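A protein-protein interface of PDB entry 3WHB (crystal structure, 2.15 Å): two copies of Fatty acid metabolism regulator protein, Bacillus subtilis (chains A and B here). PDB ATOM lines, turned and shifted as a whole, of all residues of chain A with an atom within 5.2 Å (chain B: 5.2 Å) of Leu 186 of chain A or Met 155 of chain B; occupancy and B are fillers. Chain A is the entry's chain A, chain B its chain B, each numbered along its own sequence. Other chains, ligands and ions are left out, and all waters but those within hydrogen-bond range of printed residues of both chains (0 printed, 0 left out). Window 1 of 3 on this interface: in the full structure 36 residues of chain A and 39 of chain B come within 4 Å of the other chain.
Printed residues of chain B within 4 Å of Leu 186 of chain A: Leu 147, Leu 151, Ala 152 and Met 155.
Of chain A, only Thr 159, Leu 186 and Ile 191 come within 4 Å of Met 155 of chain B.
Of the printed residues of chain B, Ser 182 of chain A touches Leu 151 (3.7 Å).
Of the printed residues of chain B, Leu 187 of chain A touches Gly 190.
Printed residues of chain A within 4 Å of Leu 151 of chain B: Ser 182 and Leu 186.
Phe 157 of chain B touches none of the printed residues of chain A.
The nearest printed residue of chain B that does not touch Leu 186 of chain A is Gly 190 of chain B (4.6 Å).
The nearest residue of chain A that does not touch Met 155 of chain B is Leu 187 of chain A (4.2 Å).
The nearest printed residue of chain A that does not touch Leu 187 of chain B is Leu 186 of chain A (5.2 Å).
Hydrophobic or aromatic side chains of chain B that line the printed part of chain A: Leu 147, Leu 151, Met 155 and Leu 187.
Along chain B the printed residues that touch a printed residue of chain A span positions 147 to 190.
Among the printed residues, 16 pairs touch across the chains.
Among the printed residues, no Asp or Glu carboxylate lies within 4 Å of a Lys or Arg side-chain nitrogen of the other chain.
OG1 of Thr 159 of chain A sits close to O of Met 155 of chain B (3.5 Å).
OG1 of Thr 159 of chain A is in hydrogen-bond range of OG1 of Thr 159 of chain B (3.1 Å).
The backbone NH of Ile 191 of chain A sits at hydrogen-bond distance from the backbone carbonyl oxygen of Leu 187 of chain B, at 3.0 Å.
O of Leu 186 of chain A lies close to SD of Met 155 of chain B, 3.8 Å away.
Met 155 of chain A touches Thr 159 of chain B, and with the chains exchanged Thr 159 of chain A touches Met 155 of chain B.
Thr 159 of chain B touches its own counterpart, Thr 159 of chain A.
Leu 187 of chain A touches Gly 190 of chain B, and with the chains exchanged Gly 190 of chain A touches Leu 187 of chain B.
Gly 190 of chain B touches its own counterpart, Gly 190 of chain A.
Positions printed for both chains: 155, 159, 187 and 190.
Of the 16 pairs that touch across the chains among the printed residues, 6 have their exchanged pair printed and touching as well.
Thr 159 of chain B touches Met 155 of chain A.
CE of Met 155 of chain A touches CD2 of Leu 187 of chain B, at 3.3 Å.
CD1 of Leu 186 of chain A touches CB of Leu 151 of chain B, 3.8 Å away.
Leu 186 of chain A touches Ala 152 of chain B (CD1 to N, 3.98 Å).
Gly 190 of chain B touches Leu 187 of chain A (CA to O, 3.3 Å).
Val 188 of chain A touches Gly 190 of chain B (O to CA, 3.5 Å).
N of Gly 190 of chain B touches C of Ser 189 of chain A, at 3.9 Å.
O of Leu 187 of chain B touches CA of Gly 190 of chain A (3.3 Å).
Gly 190 of chain A touches Gly 190 of chain B (CA to N, 3.5 Å).
Met 155 of chain B touches Ile 191 of chain A.
The backbone carbonyl oxygen of Met 155 of chain A sits at hydrogen-bond distance from the side-chain hydroxyl of Thr 159 of chain A.
The side-chain carboxylate of Asp 148 of chain B lies within hydrogen-bond range of the backbone NH of Leu 151 of chain B (2.8 Å).
O of Met 155 of chain B sits at hydrogen-bond distance from OG1 of Thr 159 of chain B (2.7 Å).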
ATOM      1  N   MET A 155       8.772  -1.740   2.247  1.00  0.00           N
ATOM      2  CA  MET A 155       7.472  -1.280   2.713  1.00  0.00           C
ATOM      3  C   MET A 155       6.568  -2.436   3.173  1.00  0.00           C
ATOM      4  O   MET A 155       6.035  -2.402   4.283  1.00  0.00           O
ATOM      5  CB  MET A 155       6.768  -0.446   1.639  1.00  0.00           C
ATOM      6  CG  MET A 155       5.259  -0.379   1.818  1.00  0.00           C
ATOM      7  SD  MET A 155       4.405   0.897   0.865  1.00  0.00           S
ATOM      8  CE  MET A 155       5.063   2.320   1.682  1.00  0.00           C
ATOM      9  N   THR A 159       5.936  -3.110   7.102  1.00  0.00           N
ATOM     10  CA  THR A 159       4.566  -2.812   7.521  1.00  0.00           C
ATOM     11  C   THR A 159       3.966  -4.011   8.255  1.00  0.00           C
ATOM     12  O   THR A 159       3.425  -3.864   9.357  1.00  0.00           O
ATOM     13  CB  THR A 159       3.681  -2.431   6.322  1.00  0.00           C
ATOM     14  OG1 THR A 159       4.062  -1.132   5.838  1.00  0.00           O
ATOM     15  CG2 THR A 159       2.203  -2.409   6.718  1.00  0.00           C
ATOM     16  N   ASN A 181      -6.593  -7.931   6.178  1.00  0.00           N
ATOM     17  CA  ASN A 181      -7.157  -7.280   5.014  1.00  0.00           C
ATOM     18  C   ASN A 181      -6.923  -5.784   5.018  1.00  0.00           C
ATOM     19  O   ASN A 181      -6.629  -5.202   3.975  1.00  0.00           O
ATOM     20  CB  ASN A 181      -8.656  -7.537   4.918  1.00  0.00           C
ATOM     21  CG  ASN A 181      -9.211  -7.116   3.584  1.00  0.00           C
ATOM     22  OD1 ASN A 181      -8.894  -7.718   2.559  1.00  0.00           O
ATOM     23  ND2 ASN A 181     -10.008  -6.061   3.576  1.00  0.00           N
ATOM     24  N   SER A 182      -7.061  -5.164   6.186  1.00  0.00           N
ATOM     25  CA  SER A 182      -6.868  -3.715   6.294  1.00  0.00           C
ATOM     26  C   SER A 182      -5.418  -3.324   6.000  1.00  0.00           C
ATOM     27  O   SER A 182      -5.166  -2.339   5.301  1.00  0.00           O
ATOM     28  CB  SER A 182      -7.306  -3.221   7.667  1.00  0.00           C
ATOM     29  OG  SER A 182      -8.710  -3.388   7.815  1.00  0.00           O
ATOM     30  N   VAL A 183      -4.478  -4.120   6.515  1.00  0.00           N
ATOM     31  CA  VAL A 183      -3.046  -3.911   6.251  1.00  0.00           C
ATOM     32  C   VAL A 183      -2.749  -4.073   4.759  1.00  0.00           C
ATOM     33  O   VAL A 183      -2.018  -3.265   4.181  1.00  0.00           O
ATOM     34  CB  VAL A 183      -2.140  -4.832   7.109  1.00  0.00           C
ATOM     35  CG1 VAL A 183      -0.690  -4.723   6.671  1.00  0.00           C
ATOM     36  CG2 VAL A 183      -2.248  -4.472   8.588  1.00  0.00           C
ATOM     37  N   LEU A 184      -3.332  -5.109   4.150  1.00  0.00           N
ATOM     38  CA  LEU A 184      -3.255  -5.315   2.707  1.00  0.00           C
ATOM     39  C   LEU A 184      -3.736  -4.080   1.918  1.00  0.00           C
ATOM     40  O   LEU A 184      -3.049  -3.623   1.009  1.00  0.00           O
ATOM     41  CB  LEU A 184      -4.071  -6.541   2.286  1.00  0.00           C
ATOM     42  CG  LEU A 184      -4.279  -6.780   0.783  1.00  0.00           C
ATOM     43  CD1 LEU A 184      -3.035  -7.352   0.123  1.00  0.00           C
ATOM     44  CD2 LEU A 184      -5.485  -7.671   0.509  1.00  0.00           C
ATOM     45  N   GLU A 185      -4.911  -3.570   2.278  1.00  0.00           N
ATOM     46  CA  GLU A 185      -5.527  -2.442   1.578  1.00  0.00           C
ATOM     47  C   GLU A 185      -4.709  -1.157   1.716  1.00  0.00           C
ATOM     48  O   GLU A 185      -4.620  -0.384   0.766  1.00  0.00           O
ATOM     49  CB  GLU A 185      -6.971  -2.221   2.050  1.00  0.00           C
ATOM     50  CG  GLU A 185      -7.940  -3.336   1.663  1.00  0.00           C
ATOM     51  CD  GLU A 185      -8.314  -3.344   0.184  1.00  0.00           C
ATOM     52  OE1 GLU A 185      -7.940  -2.399  -0.554  1.00  0.00           O
ATOM     53  OE2 GLU A 185      -8.994  -4.304  -0.244  1.00  0.00           O
ATOM     54  N   LEU A 186      -4.116  -0.944   2.893  1.00  0.00           N
ATOM     55  CA  LEU A 186      -3.170   0.156   3.106  1.00  0.00           C
ATOM     56  C   LEU A 186      -1.958   0.051   2.185  1.00  0.00           C
ATOM     57  O   LEU A 186      -1.548   1.039   1.573  1.00  0.00           O
ATOM     58  CB  LEU A 186      -2.689   0.199   4.558  1.00  0.00           C
ATOM     59  CG  LEU A 186      -3.617   0.858   5.577  1.00  0.00           C
ATOM     60  CD1 LEU A 186      -3.204   0.485   6.990  1.00  0.00           C
ATOM     61  CD2 LEU A 186      -3.637   2.371   5.391  1.00  0.00           C
ATOM     62  N   LEU A 187      -1.394  -1.153   2.089  1.00  0.00           N
ATOM     63  CA  LEU A 187      -0.221  -1.387   1.254  1.00  0.00           C
ATOM     64  C   LEU A 187      -0.548  -1.234  -0.232  1.00  0.00           C
ATOM     65  O   LEU A 187       0.282  -0.756  -1.012  1.00  0.00           O
ATOM     66  CB  LEU A 187       0.353  -2.779   1.531  1.00  0.00           C
ATOM     67  CG  LEU A 187       1.087  -2.969   2.862  1.00  0.00           C
ATOM     68  CD1 LEU A 187       1.359  -4.442   3.126  1.00  0.00           C
ATOM     69  CD2 LEU A 187       2.383  -2.172   2.871  1.00  0.00           C
ATOM     70  N   VAL A 188      -1.762  -1.625  -0.611  1.00  0.00           N
ATOM     71  CA  VAL A 188      -2.182  -1.615  -2.011  1.00  0.00           C
ATOM     72  C   VAL A 188      -2.552  -0.204  -2.470  1.00  0.00           C
ATOM     73  O   VAL A 188      -2.138   0.228  -3.550  1.00  0.00           O
ATOM     74  CB  VAL A 188      -3.328  -2.629  -2.267  1.00  0.00           C
ATOM     75  CG1 VAL A 188      -4.081  -2.325  -3.560  1.00  0.00           C
ATOM     76  CG2 VAL A 188      -2.767  -4.043  -2.308  1.00  0.00           C
ATOM     77  N   SER A 189      -3.309   0.514  -1.643  1.00  0.00           N
ATOM     78  CA  SER A 189      -3.834   1.829  -2.025  1.00  0.00           C
ATOM     79  C   SER A 189      -3.137   3.040  -1.405  1.00  0.00           C
ATOM     80  O   SER A 189      -3.381   4.173  -1.834  1.00  0.00           O
ATOM     81  CB  SER A 189      -5.339   1.908  -1.739  1.00  0.00           C
ATOM     82  OG  SER A 189      -6.069   1.281  -2.772  1.00  0.00           O
ATOM     83  N   GLY A 190      -2.281   2.815  -0.410  1.00  0.00           N
ATOM     84  CA  GLY A 190      -1.618   3.926   0.279  1.00  0.00           C
ATOM     85  C   GLY A 190      -2.571   4.660   1.209  1.00  0.00           C
ATOM     86  O   GLY A 190      -3.713   4.236   1.392  1.00  0.00           O
ATOM     87  N   ILE A 191      -2.105   5.759   1.795  1.00  0.00           N
ATOM     88  CA  ILE A 191      -2.917   6.534   2.737  1.00  0.00           C
ATOM     89  C   ILE A 191      -3.816   7.590   2.084  1.00  0.00           C
ATOM     90  O   ILE A 191      -4.769   8.051   2.707  1.00  0.00           O
ATOM     91  CB  ILE A 191      -2.068   7.216   3.842  1.00  0.00           C
ATOM     92  CG1 ILE A 191      -0.955   8.074   3.227  1.00  0.00           C
ATOM     93  CG2 ILE A 191      -1.528   6.183   4.821  1.00  0.00           C
ATOM     94  CD1 ILE A 191      -0.132   8.846   4.238  1.00  0.00           C
ATOM     95  N   LEU B 147      -9.820   5.695   7.396  1.00  0.00           N
ATOM     96  CA  LEU B 147      -8.485   5.183   7.693  1.00  0.00           C
ATOM     97  C   LEU B 147      -8.325   4.815   9.168  1.00  0.00           C
ATOM     98  O   LEU B 147      -8.656   5.607  10.047  1.00  0.00           O
ATOM     99  CB  LEU B 147      -7.441   6.244   7.340  1.00  0.00           C
ATOM    100  CG  LEU B 147      -5.956   5.902   7.486  1.00  0.00           C
ATOM    101  CD1 LEU B 147      -5.426   5.337   6.180  1.00  0.00           C
ATOM    102  CD2 LEU B 147      -5.185   7.151   7.875  1.00  0.00           C
ATOM    103  N   ASP B 148      -7.821   3.615   9.430  1.00  0.00           N
ATOM    104  CA  ASP B 148      -7.447   3.236  10.791  1.00  0.00           C
ATOM    105  C   ASP B 148      -6.127   3.912  11.087  1.00  0.00           C
ATOM    106  O   ASP B 148      -5.089   3.504  10.569  1.00  0.00           O
ATOM    107  CB  ASP B 148      -7.317   1.717  10.929  1.00  0.00           C
ATOM    108  CG  ASP B 148      -7.026   1.282  12.357  1.00  0.00           C
ATOM    109  OD1 ASP B 148      -6.014   1.725  12.932  1.00  0.00           O
ATOM    110  OD2 ASP B 148      -7.810   0.483  12.901  1.00  0.00           O
ATOM    111  N   LEU B 151      -3.256   1.761  12.513  1.00  0.00           N
ATOM    112  CA  LEU B 151      -2.696   0.885  11.486  1.00  0.00           C
ATOM    113  C   LEU B 151      -1.813   1.617  10.487  1.00  0.00           C
ATOM    114  O   LEU B 151      -0.765   1.108  10.091  1.00  0.00           O
ATOM    115  CB  LEU B 151      -3.796   0.138  10.742  1.00  0.00           C
ATOM    116  CG  LEU B 151      -4.328  -1.133  11.397  1.00  0.00           C
ATOM    117  CD1 LEU B 151      -5.313  -1.774  10.438  1.00  0.00           C
ATOM    118  CD2 LEU B 151      -3.206  -2.101  11.748  1.00  0.00           C
ATOM    119  N   ALA B 152      -2.243   2.807  10.082  1.00  0.00           N
ATOM    120  CA  ALA B 152      -1.507   3.580   9.090  1.00  0.00           C
ATOM    121  C   ALA B 152      -0.181   4.071   9.660  1.00  0.00           C
ATOM    122  O   ALA B 152       0.830   4.098   8.960  1.00  0.00           O
ATOM    123  CB  ALA B 152      -2.352   4.743   8.580  1.00  0.00           C
ATOM    124  N   ARG B 153      -0.196   4.441  10.936  1.00  0.00           N
ATOM    125  CA  ARG B 153       1.006   4.866  11.647  1.00  0.00           C
ATOM    126  C   ARG B 153       1.985   3.702  11.739  1.00  0.00           C
ATOM    127  O   ARG B 153       3.185   3.878  11.529  1.00  0.00           O
ATOM    128  CB  ARG B 153       0.636   5.397  13.038  1.00  0.00           C
ATOM    129  CG  ARG B 153       1.794   5.509  14.019  1.00  0.00           C
ATOM    130  CD  ARG B 153       1.678   4.478  15.132  1.00  0.00           C
ATOM    131  NE  ARG B 153       0.601   4.816  16.062  1.00  0.00           N
ATOM    132  CZ  ARG B 153       0.049   3.968  16.921  1.00  0.00           C
ATOM    133  NH1 ARG B 153       0.480   2.708  16.998  1.00  0.00           N
ATOM    134  NH2 ARG B 153      -0.929   4.382  17.711  1.00  0.00           N
ATOM    135  N   GLN B 154       1.464   2.513  12.044  1.00  0.00           N
ATOM    136  CA  GLN B 154       2.272   1.298  12.030  1.00  0.00           C
ATOM    137  C   GLN B 154       2.930   1.073  10.665  1.00  0.00           C
ATOM    138  O   GLN B 154       4.108   0.737  10.597  1.00  0.00           O
ATOM    139  CB  GLN B 154       1.435   0.088  12.467  1.00  0.00           C
ATOM    140  CG  GLN B 154       1.228   0.028  13.978  1.00  0.00           C
ATOM    141  CD  GLN B 154       0.087  -0.881  14.384  1.00  0.00           C
ATOM    142  OE1 GLN B 154       0.195  -2.108  14.302  1.00  0.00           O
ATOM    143  NE2 GLN B 154      -1.016  -0.286  14.839  1.00  0.00           N
ATOM    144  N   MET B 155       2.176   1.285   9.586  1.00  0.00           N
ATOM    145  CA  MET B 155       2.714   1.123   8.236  1.00  0.00           C
ATOM    146  C   MET B 155       3.806   2.157   7.933  1.00  0.00           C
ATOM    147  O   MET B 155       4.888   1.812   7.441  1.00  0.00           O
ATOM    148  CB  MET B 155       1.598   1.208   7.184  1.00  0.00           C
ATOM    149  CG  MET B 155       2.116   1.342   5.754  1.00  0.00           C
ATOM    150  SD  MET B 155       0.885   1.509   4.445  1.00  0.00           S
ATOM    151  CE  MET B 155       0.429   3.222   4.653  1.00  0.00           C
ATOM    152  N   ILE B 156       3.508   3.422   8.221  1.00  0.00           N
ATOM    153  CA  ILE B 156       4.449   4.505   7.988  1.00  0.00           C
ATOM    154  C   ILE B 156       5.741   4.296   8.776  1.00  0.00           C
ATOM    155  O   ILE B 156       6.825   4.265   8.195  1.00  0.00           O
ATOM    156  CB  ILE B 156       3.820   5.882   8.289  1.00  0.00           C
ATOM    157  CG1 ILE B 156       2.741   6.203   7.251  1.00  0.00           C
ATOM    158  CG2 ILE B 156       4.887   6.966   8.291  1.00  0.00           C
ATOM    159  CD1 ILE B 156       1.770   7.284   7.674  1.00  0.00           C
ATOM    160  N   PHE B 157       5.620   4.134  10.091  1.00  0.00           N
ATOM    161  CA  PHE B 157       6.789   3.887  10.928  1.00  0.00           C
ATOM    162  C   PHE B 157       7.517   2.608  10.514  1.00  0.00           C
ATOM    163  O   PHE B 157       8.741   2.605  10.398  1.00  0.00           O
ATOM    164  CB  PHE B 157       6.425   3.823  12.414  1.00  0.00           C
ATOM    165  CG  PHE B 157       7.626   3.746  13.312  1.00  0.00           C
ATOM    166  CD1 PHE B 157       8.080   2.524  13.783  1.00  0.00           C
ATOM    167  CD2 PHE B 157       8.334   4.898  13.648  1.00  0.00           C
ATOM    168  CE1 PHE B 157       9.204   2.451  14.593  1.00  0.00           C
ATOM    169  CE2 PHE B 157       9.457   4.832  14.459  1.00  0.00           C
ATOM    170  CZ  PHE B 157       9.894   3.605  14.935  1.00  0.00           C
ATOM    171  N   GLY B 158       6.761   1.533  10.294  1.00  0.00           N
ATOM    172  CA  GLY B 158       7.346   0.246   9.922  1.00  0.00           C
ATOM    173  C   GLY B 158       8.144   0.321   8.642  1.00  0.00           C
ATOM    174  O   GLY B 158       9.212  -0.271   8.540  1.00  0.00           O
ATOM    175  N   THR B 159       7.611   1.064   7.672  1.00  0.00           N
ATOM    176  CA  THR B 159       8.247   1.276   6.376  1.00  0.00           C
ATOM    177  C   THR B 159       9.528   2.099   6.503  1.00  0.00           C
ATOM    178  O   THR B 159      10.568   1.715   5.972  1.00  0.00           O
ATOM    179  CB  THR B 159       7.256   1.932   5.392  1.00  0.00           C
ATOM    180  OG1 THR B 159       6.166   1.033   5.163  1.00  0.00           O
ATOM    181  CG2 THR B 159       7.930   2.310   4.043  1.00  0.00           C
ATOM    182  N   ILE B 160       9.452   3.221   7.215  1.00  0.00           N
ATOM    183  CA  ILE B 160      10.630   4.039   7.468  1.00  0.00           C
ATOM    184  C   ILE B 160      11.723   3.203   8.142  1.00  0.00           C
ATOM    185  O   ILE B 160      12.865   3.164   7.678  1.00  0.00           O
ATOM    186  CB  ILE B 160      10.302   5.275   8.334  1.00  0.00           C
ATOM    187  CG1 ILE B 160       9.335   6.209   7.596  1.00  0.00           C
ATOM    188  CG2 ILE B 160      11.582   6.020   8.697  1.00  0.00           C
ATOM    189  CD1 ILE B 160       8.714   7.280   8.475  1.00  0.00           C
ATOM    190  N   LEU B 187       4.124   5.204   0.324  1.00  0.00           N
ATOM    191  CA  LEU B 187       3.234   5.283   1.481  1.00  0.00           C
ATOM    192  C   LEU B 187       1.931   5.980   1.127  1.00  0.00           C
ATOM    193  O   LEU B 187       0.872   5.619   1.636  1.00  0.00           O
ATOM    194  CB  LEU B 187       3.915   5.989   2.670  1.00  0.00           C
ATOM    195  CG  LEU B 187       4.919   5.159   3.492  1.00  0.00           C
ATOM    196  CD1 LEU B 187       5.807   6.048   4.349  1.00  0.00           C
ATOM    197  CD2 LEU B 187       4.236   4.096   4.349  1.00  0.00           C
ATOM    198  N   GLY B 190       0.549   3.649  -2.474  1.00  0.00           N
ATOM    199  CA  GLY B 190       0.553   2.190  -2.404  1.00  0.00           C
ATOM    200  C   GLY B 190       1.168   1.576  -3.650  1.00  0.00           C
ATOM    201  O   GLY B 190       1.826   2.269  -4.435  1.00  0.00           O
